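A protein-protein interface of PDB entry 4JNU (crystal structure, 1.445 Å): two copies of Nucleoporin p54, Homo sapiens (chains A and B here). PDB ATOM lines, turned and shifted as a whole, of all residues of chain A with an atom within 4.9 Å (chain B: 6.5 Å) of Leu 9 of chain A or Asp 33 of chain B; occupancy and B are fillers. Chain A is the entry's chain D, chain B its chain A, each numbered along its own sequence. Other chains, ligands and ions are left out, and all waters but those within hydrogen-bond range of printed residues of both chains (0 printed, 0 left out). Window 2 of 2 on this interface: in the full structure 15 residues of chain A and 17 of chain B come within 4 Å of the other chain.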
ATOM      1  N   TYR A   3     -33.391   6.378 -18.704  1.00  0.00           N
ATOM      2  CA  TYR A   3     -31.995   5.969 -18.745  1.00  0.00           C
ATOM      3  C   TYR A   3     -31.180   7.158 -19.212  1.00  0.00           C
ATOM      4  O   TYR A   3     -31.244   7.551 -20.380  1.00  0.00           O
ATOM      5  CB  TYR A   3     -31.769   4.773 -19.675  1.00  0.00           C
ATOM      6  CG  TYR A   3     -30.293   4.413 -19.838  1.00  0.00           C
ATOM      7  CD1 TYR A   3     -29.476   4.259 -18.729  1.00  0.00           C
ATOM      8  CD2 TYR A   3     -29.736   4.198 -21.092  1.00  0.00           C
ATOM      9  CE1 TYR A   3     -28.143   3.928 -18.859  1.00  0.00           C
ATOM     10  CE2 TYR A   3     -28.392   3.871 -21.237  1.00  0.00           C
ATOM     11  CZ  TYR A   3     -27.601   3.727 -20.113  1.00  0.00           C
ATOM     12  OH  TYR A   3     -26.271   3.399 -20.237  1.00  0.00           O
ATOM     13  N   ASP A   5     -28.191   7.773 -20.051  1.00  0.00           N
ATOM     14  CA  ASP A   5     -27.212   7.650 -21.143  1.00  0.00           C
ATOM     15  C   ASP A   5     -27.761   7.040 -22.420  1.00  0.00           C
ATOM     16  O   ASP A   5     -26.990   6.602 -23.274  1.00  0.00           O
ATOM     17  CB  ASP A   5     -26.014   6.825 -20.664  1.00  0.00           C
ATOM     18  CG  ASP A   5     -25.228   7.520 -19.585  1.00  0.00           C
ATOM     19  OD1 ASP A   5     -25.103   8.763 -19.641  1.00  0.00           O
ATOM     20  OD2 ASP A   5     -24.734   6.826 -18.667  1.00  0.00           O
ATOM     21  N   ALA A   6     -29.079   7.019 -22.569  1.00  0.00           N
ATOM     22  CA  ALA A   6     -29.688   6.403 -23.741  1.00  0.00           C
ATOM     23  C   ALA A   6     -29.236   7.082 -25.018  1.00  0.00           C
ATOM     24  O   ALA A   6     -28.834   6.401 -25.950  1.00  0.00           O
ATOM     25  CB  ALA A   6     -31.196   6.418 -23.642  1.00  0.00           C
ATOM     26  N   ASP A   7     -29.335   8.406 -25.070  1.00  0.00           N
ATOM     27  CA  ASP A   7     -28.943   9.137 -26.271  1.00  0.00           C
ATOM     28  C   ASP A   7     -27.466   8.952 -26.525  1.00  0.00           C
ATOM     29  O   ASP A   7     -27.062   8.796 -27.668  1.00  0.00           O
ATOM     30  CB  ASP A   7     -29.271  10.624 -26.139  1.00  0.00           C
ATOM     31  CG  ASP A   7     -30.758  10.910 -26.276  1.00  0.00           C
ATOM     32  OD1 ASP A   7     -31.464  10.095 -26.907  1.00  0.00           O
ATOM     33  OD2 ASP A   7     -31.217  11.956 -25.769  1.00  0.00           O
ATOM     34  N   LEU A   8     -26.659   8.956 -25.474  1.00  0.00           N
ATOM     35  CA  LEU A   8     -25.224   8.731 -25.633  1.00  0.00           C
ATOM     36  C   LEU A   8     -24.919   7.367 -26.215  1.00  0.00           C
ATOM     37  O   LEU A   8     -24.086   7.255 -27.133  1.00  0.00           O
ATOM     38  CB  LEU A   8     -24.510   8.905 -24.297  1.00  0.00           C
ATOM     39  CG  LEU A   8     -23.010   8.636 -24.303  1.00  0.00           C
ATOM     40  CD1 LEU A   8     -22.282   9.560 -25.276  1.00  0.00           C
ATOM     41  CD2 LEU A   8     -22.419   8.755 -22.912  1.00  0.00           C
ATOM     42  N   LEU A   9     -25.568   6.316 -25.729  1.00  0.00           N
ATOM     43  CA  LEU A   9     -25.308   4.993 -26.261  1.00  0.00           C
ATOM     44  C   LEU A   9     -25.706   4.925 -27.731  1.00  0.00           C
ATOM     45  O   LEU A   9     -24.996   4.318 -28.534  1.00  0.00           O
ATOM     46  CB  LEU A   9     -26.053   3.901 -25.488  1.00  0.00           C
ATOM     47  CG  LEU A   9     -25.626   3.582 -24.057  1.00  0.00           C
ATOM     48  CD1 LEU A   9     -26.291   2.276 -23.612  1.00  0.00           C
ATOM     49  CD2 LEU A   9     -24.133   3.494 -23.896  1.00  0.00           C
ATOM     50  N   ARG A  10     -26.830   5.535 -28.086  1.00  0.00           N
ATOM     51  CA  ARG A  10     -27.250   5.571 -29.482  1.00  0.00           C
ATOM     52  C   ARG A  10     -26.209   6.275 -30.345  1.00  0.00           C
ATOM     53  O   ARG A  10     -25.905   5.836 -31.461  1.00  0.00           O
ATOM     54  CB  ARG A  10     -28.609   6.260 -29.609  1.00  0.00           C
ATOM     55  CG  ARG A  10     -29.746   5.503 -28.955  1.00  0.00           C
ATOM     56  CD  ARG A  10     -31.056   6.263 -29.076  1.00  0.00           C
ATOM     57  NE  ARG A  10     -32.127   5.656 -28.287  1.00  0.00           N
ATOM     58  CZ  ARG A  10     -32.737   6.230 -27.250  1.00  0.00           C
ATOM     59  NH1 ARG A  10     -32.408   7.450 -26.848  1.00  0.00           N
ATOM     60  NH2 ARG A  10     -33.698   5.578 -26.613  1.00  0.00           N
ATOM     61  N   GLU A  11     -25.657   7.373 -29.842  1.00  0.00           N
ATOM     62  CA  GLU A  11     -24.660   8.135 -30.602  1.00  0.00           C
ATOM     63  C   GLU A  11     -23.368   7.357 -30.760  1.00  0.00           C
ATOM     64  O   GLU A  11     -22.745   7.355 -31.827  1.00  0.00           O
ATOM     65  CB  GLU A  11     -24.378   9.465 -29.896  1.00  0.00           C
ATOM     66  CG  GLU A  11     -25.521  10.467 -29.992  1.00  0.00           C
ATOM     67  CD  GLU A  11     -25.195  11.801 -29.344  1.00  0.00           C
ATOM     68  OE1 GLU A  11     -24.535  11.812 -28.280  1.00  0.00           O
ATOM     69  OE2 GLU A  11     -25.606  12.843 -29.903  1.00  0.00           O
ATOM     70  N   ILE A  12     -22.915   6.716 -29.689  1.00  0.00           N
ATOM     71  CA  ILE A  12     -21.718   5.885 -29.746  1.00  0.00           C
ATOM     72  C   ILE A  12     -21.923   4.767 -30.764  1.00  0.00           C
ATOM     73  O   ILE A  12     -21.057   4.546 -31.624  1.00  0.00           O
ATOM     74  CB  ILE A  12     -21.368   5.273 -28.374  1.00  0.00           C
ATOM     75  CG1 ILE A  12     -20.933   6.365 -27.391  1.00  0.00           C
ATOM     76  CG2 ILE A  12     -20.236   4.293 -28.522  1.00  0.00           C
ATOM     77  CD1 ILE A  12     -20.926   5.905 -25.953  1.00  0.00           C
ATOM     78  N   LYS A  13     -23.069   4.098 -30.721  1.00  0.00           N
ATOM     79  CA  LYS A  13     -23.325   3.024 -31.682  1.00  0.00           C
ATOM     80  C   LYS A  13     -23.307   3.548 -33.114  1.00  0.00           C
ATOM     81  O   LYS A  13     -22.741   2.900 -34.000  1.00  0.00           O
ATOM     82  CB  LYS A  13     -24.648   2.320 -31.362  1.00  0.00           C
ATOM     83  CG  LYS A  13     -24.946   1.158 -32.316  1.00  0.00           C
ATOM     84  CD  LYS A  13     -25.845   0.069 -31.685  1.00  0.00           C
ATOM     85  CE  LYS A  13     -27.113   0.620 -31.069  1.00  0.00           C
ATOM     86  NZ  LYS A  13     -28.009   1.289 -32.043  1.00  0.00           N
ATOM     87  N   SER B  28     -22.428  -5.023 -30.670  1.00  0.00           N
ATOM     88  CA  SER B  28     -23.305  -6.017 -30.056  1.00  0.00           C
ATOM     89  C   SER B  28     -23.531  -5.724 -28.574  1.00  0.00           C
ATOM     90  O   SER B  28     -24.642  -5.865 -28.065  1.00  0.00           O
ATOM     91  CB  SER B  28     -22.710  -7.408 -30.222  1.00  0.00           C
ATOM     92  OG  SER B  28     -22.794  -7.817 -31.574  1.00  0.00           O
ATOM     93  N   ILE B  29     -22.477  -5.340 -27.869  1.00  0.00           N
ATOM     94  CA  ILE B  29     -22.581  -5.035 -26.449  1.00  0.00           C
ATOM     95  C   ILE B  29     -23.508  -3.862 -26.217  1.00  0.00           C
ATOM     96  O   ILE B  29     -24.352  -3.905 -25.331  1.00  0.00           O
ATOM     97  CB  ILE B  29     -21.189  -4.764 -25.868  1.00  0.00           C
ATOM     98  CG1 ILE B  29     -20.443  -6.080 -25.670  1.00  0.00           C
ATOM     99  CG2 ILE B  29     -21.279  -4.032 -24.531  1.00  0.00           C
ATOM    100  CD1 ILE B  29     -18.932  -5.884 -25.455  1.00  0.00           C
ATOM    101  N   ILE B  30     -23.385  -2.822 -27.024  1.00  0.00           N
ATOM    102  CA  ILE B  30     -24.246  -1.655 -26.884  1.00  0.00           C
ATOM    103  C   ILE B  30     -25.699  -1.994 -27.242  1.00  0.00           C
ATOM    104  O   ILE B  30     -26.621  -1.551 -26.559  1.00  0.00           O
ATOM    105  CB  ILE B  30     -23.708  -0.488 -27.734  1.00  0.00           C
ATOM    106  CG1 ILE B  30     -22.356  -0.049 -27.163  1.00  0.00           C
ATOM    107  CG2 ILE B  30     -24.697   0.685 -27.742  1.00  0.00           C
ATOM    108  CD1 ILE B  30     -21.573   0.871 -28.065  1.00  0.00           C
ATOM    109  N   LYS B  31     -25.899  -2.765 -28.305  1.00  0.00           N
ATOM    110  CA  LYS B  31     -27.238  -3.185 -28.666  1.00  0.00           C
ATOM    111  C   LYS B  31     -27.879  -3.924 -27.499  1.00  0.00           C
ATOM    112  O   LYS B  31     -29.062  -3.707 -27.181  1.00  0.00           O
ATOM    113  CB  LYS B  31     -27.211  -4.062 -29.905  1.00  0.00           C
ATOM    114  CG  LYS B  31     -26.999  -3.274 -31.190  1.00  0.00           C
ATOM    115  CD  LYS B  31     -26.991  -4.165 -32.421  1.00  0.00           C
ATOM    116  CE  LYS B  31     -26.873  -3.351 -33.701  1.00  0.00           C
ATOM    117  NZ  LYS B  31     -26.778  -4.204 -34.922  1.00  0.00           N
ATOM    118  N   ASP B  32     -27.118  -4.808 -26.850  1.00  0.00           N
ATOM    119  CA  ASP B  32     -27.660  -5.571 -25.721  1.00  0.00           C
ATOM    120  C   ASP B  32     -27.971  -4.661 -24.540  1.00  0.00           C
ATOM    121  O   ASP B  32     -28.984  -4.852 -23.855  1.00  0.00           O
ATOM    122  CB  ASP B  32     -26.697  -6.680 -25.295  1.00  0.00           C
ATOM    123  CG  ASP B  32     -26.564  -7.769 -26.342  1.00  0.00           C
ATOM    124  OD1 ASP B  32     -27.403  -7.810 -27.269  1.00  0.00           O
ATOM    125  OD2 ASP B  32     -25.629  -8.591 -26.230  1.00  0.00           O
ATOM    126  N   ASP B  33     -27.117  -3.674 -24.302  1.00  0.00           N
ATOM    127  CA  ASP B  33     -27.338  -2.690 -23.246  1.00  0.00           C
ATOM    128  C   ASP B  33     -28.661  -1.981 -23.487  1.00  0.00           C
ATOM    129  O   ASP B  33     -29.449  -1.801 -22.574  1.00  0.00           O
ATOM    130  CB  ASP B  33     -26.220  -1.629 -23.237  1.00  0.00           C
ATOM    131  CG  ASP B  33     -24.873  -2.153 -22.736  1.00  0.00           C
ATOM    132  OD1 ASP B  33     -24.806  -3.228 -22.105  1.00  0.00           O
ATOM    133  OD2 ASP B  33     -23.857  -1.444 -22.964  1.00  0.00           O
ATOM    134  N   LEU B  34     -28.884  -1.555 -24.720  1.00  0.00           N
ATOM    135  CA  LEU B  34     -30.085  -0.813 -25.080  1.00  0.00           C
ATOM    136  C   LEU B  34     -31.346  -1.661 -25.013  1.00  0.00           C
ATOM    137  O   LEU B  34     -32.417  -1.135 -24.698  1.00  0.00           O
ATOM    138  CB  LEU B  34     -29.931  -0.189 -26.467  1.00  0.00           C
ATOM    139  CG  LEU B  34     -28.966   1.004 -26.507  1.00  0.00           C
ATOM    140  CD1 LEU B  34     -28.650   1.386 -27.930  1.00  0.00           C
ATOM    141  CD2 LEU B  34     -29.554   2.192 -25.757  1.00  0.00           C
ATOM    142  N   GLU B  35     -31.237  -2.959 -25.287  1.00  0.00           N
ATOM    143  CA  GLU B  35     -32.380  -3.853 -25.097  1.00  0.00           C
ATOM    144  C   GLU B  35     -32.727  -3.944 -23.618  1.00  0.00           C
ATOM    145  O   GLU B  35     -33.900  -3.946 -23.234  1.00  0.00           O
ATOM    146  CB  GLU B  35     -32.074  -5.254 -25.632  1.00  0.00           C
ATOM    147  CG  GLU B  35     -32.003  -5.323 -27.130  1.00  0.00           C
ATOM    148  CD  GLU B  35     -33.241  -4.757 -27.784  1.00  0.00           C
ATOM    149  OE1 GLU B  35     -34.351  -5.128 -27.354  1.00  0.00           O
ATOM    150  OE2 GLU B  35     -33.106  -3.935 -28.716  1.00  0.00           O
ATOM    151  N   ASP B  36     -31.701  -4.035 -22.784  1.00  0.00           N
ATOM    152  CA  ASP B  36     -31.898  -4.232 -21.360  1.00  0.00           C
ATOM    153  C   ASP B  36     -32.519  -3.001 -20.716  1.00  0.00           C
ATOM    154  O   ASP B  36     -33.323  -3.109 -19.783  1.00  0.00           O
ATOM    155  CB  ASP B  36     -30.569  -4.569 -20.689  1.00  0.00           C
ATOM    156  CG  ASP B  36     -30.094  -5.971 -21.012  1.00  0.00           C
ATOM    157  OD1 ASP B  36     -30.846  -6.716 -21.676  1.00  0.00           O
ATOM    158  OD2 ASP B  36     -28.973  -6.333 -20.592  1.00  0.00           O
ATOM    159  N   ILE B  37     -32.159  -1.827 -21.216  1.00  0.00           N
ATOM    160  CA  ILE B  37     -32.697  -0.586 -20.673  1.00  0.00           C
ATOM    161  C   ILE B  37     -34.208  -0.468 -20.910  1.00  0.00           C
ATOM    162  O   ILE B  37     -34.888   0.320 -20.249  1.00  0.00           O
ATOM    163  CB  ILE B  37     -31.963   0.641 -21.256  1.00  0.00           C
ATOM    164  CG1 ILE B  37     -31.396   1.497 -20.130  1.00  0.00           C
ATOM    165  CG2 ILE B  37     -32.890   1.473 -22.130  1.00  0.00           C
ATOM    166  CD1 ILE B  37     -30.139   0.930 -19.507  1.00  0.00           C
ATOM    167  N   LYS B  38     -34.750  -1.257 -21.833  1.00  0.00           N
ATOM    168  CA  LYS B  38     -36.190  -1.234 -22.070  1.00  0.00           C
ATOM    169  C   LYS B  38     -36.990  -1.685 -20.854  1.00  0.00           C
ATOM    170  O   LYS B  38     -38.164  -1.350 -20.720  1.00  0.00           O
ATOM    171  CB  LYS B  38     -36.545  -2.147 -23.235  1.00  0.00           C
ATOM    172  CG  LYS B  38     -36.000  -1.693 -24.553  1.00  0.00           C
ATOM    173  CD  LYS B  38     -36.354  -2.701 -25.615  1.00  0.00           C
ATOM    174  CE  LYS B  38     -35.954  -2.233 -26.986  1.00  0.00           C
ATOM    175  NZ  LYS B  38     -36.131  -3.358 -27.930  1.00  0.00           N
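Among the printed residues, pairs that only touch across the chains: Tyr 3 of chain A with Ile 37 of chain B, Leu 9 of chain A with Ile 30 of chain B, Leu 9 of chain A with Asp 33 of chain B, Leu 9 of chain A with Leu 34 of chain B, Ile 12 of chain A with Ile 30 of chain B, Lys 13 of chain A with Ile 30 of chain B, Lys 13 of chain A with Lys 31 of chain B and Lys 13 of chain A with Leu 34 of chain B.
Asp 7 of chain A touches none of the printed residues of chain B.
Arg 10 of chain A touches none of the printed residues of chain B.
Of the printed residues of chain B, Lys 13 of chain A touches Ile 30 (3.97 Å), Lys 31 (3.6 Å) and Leu 34 (3.6 Å).
Of the printed residues of chain A, Ile 30 of chain B touches Leu 9, Ile 12 and Lys 13.
Of the printed residues of chain A, Lys 31 of chain B touches Lys 13.
Printed residues of chain A within 4 Å of Leu 34 of chain B: Leu 9 and Lys 13.
The nearest printed residue of chain A that does not touch Lys 31 of chain B is Leu 9 of chain A (6.9 Å).
Hydrophobic or aromatic side chains of chain B within 4 Å of the printed part of chain A: Ile 30, Leu 34 and Ile 37.
Along chain B the printed residues that touch a printed residue of chain A span positions 30 to 37.
Hydrophobic or aromatic side chains of chain A that line the printed part of chain B: Tyr 3, Leu 9 and Ile 12.
No position is printed for both chains.
Of the 8 pairs that touch across the chains among the printed residues, none has its exchanged pair printed and touching as well.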
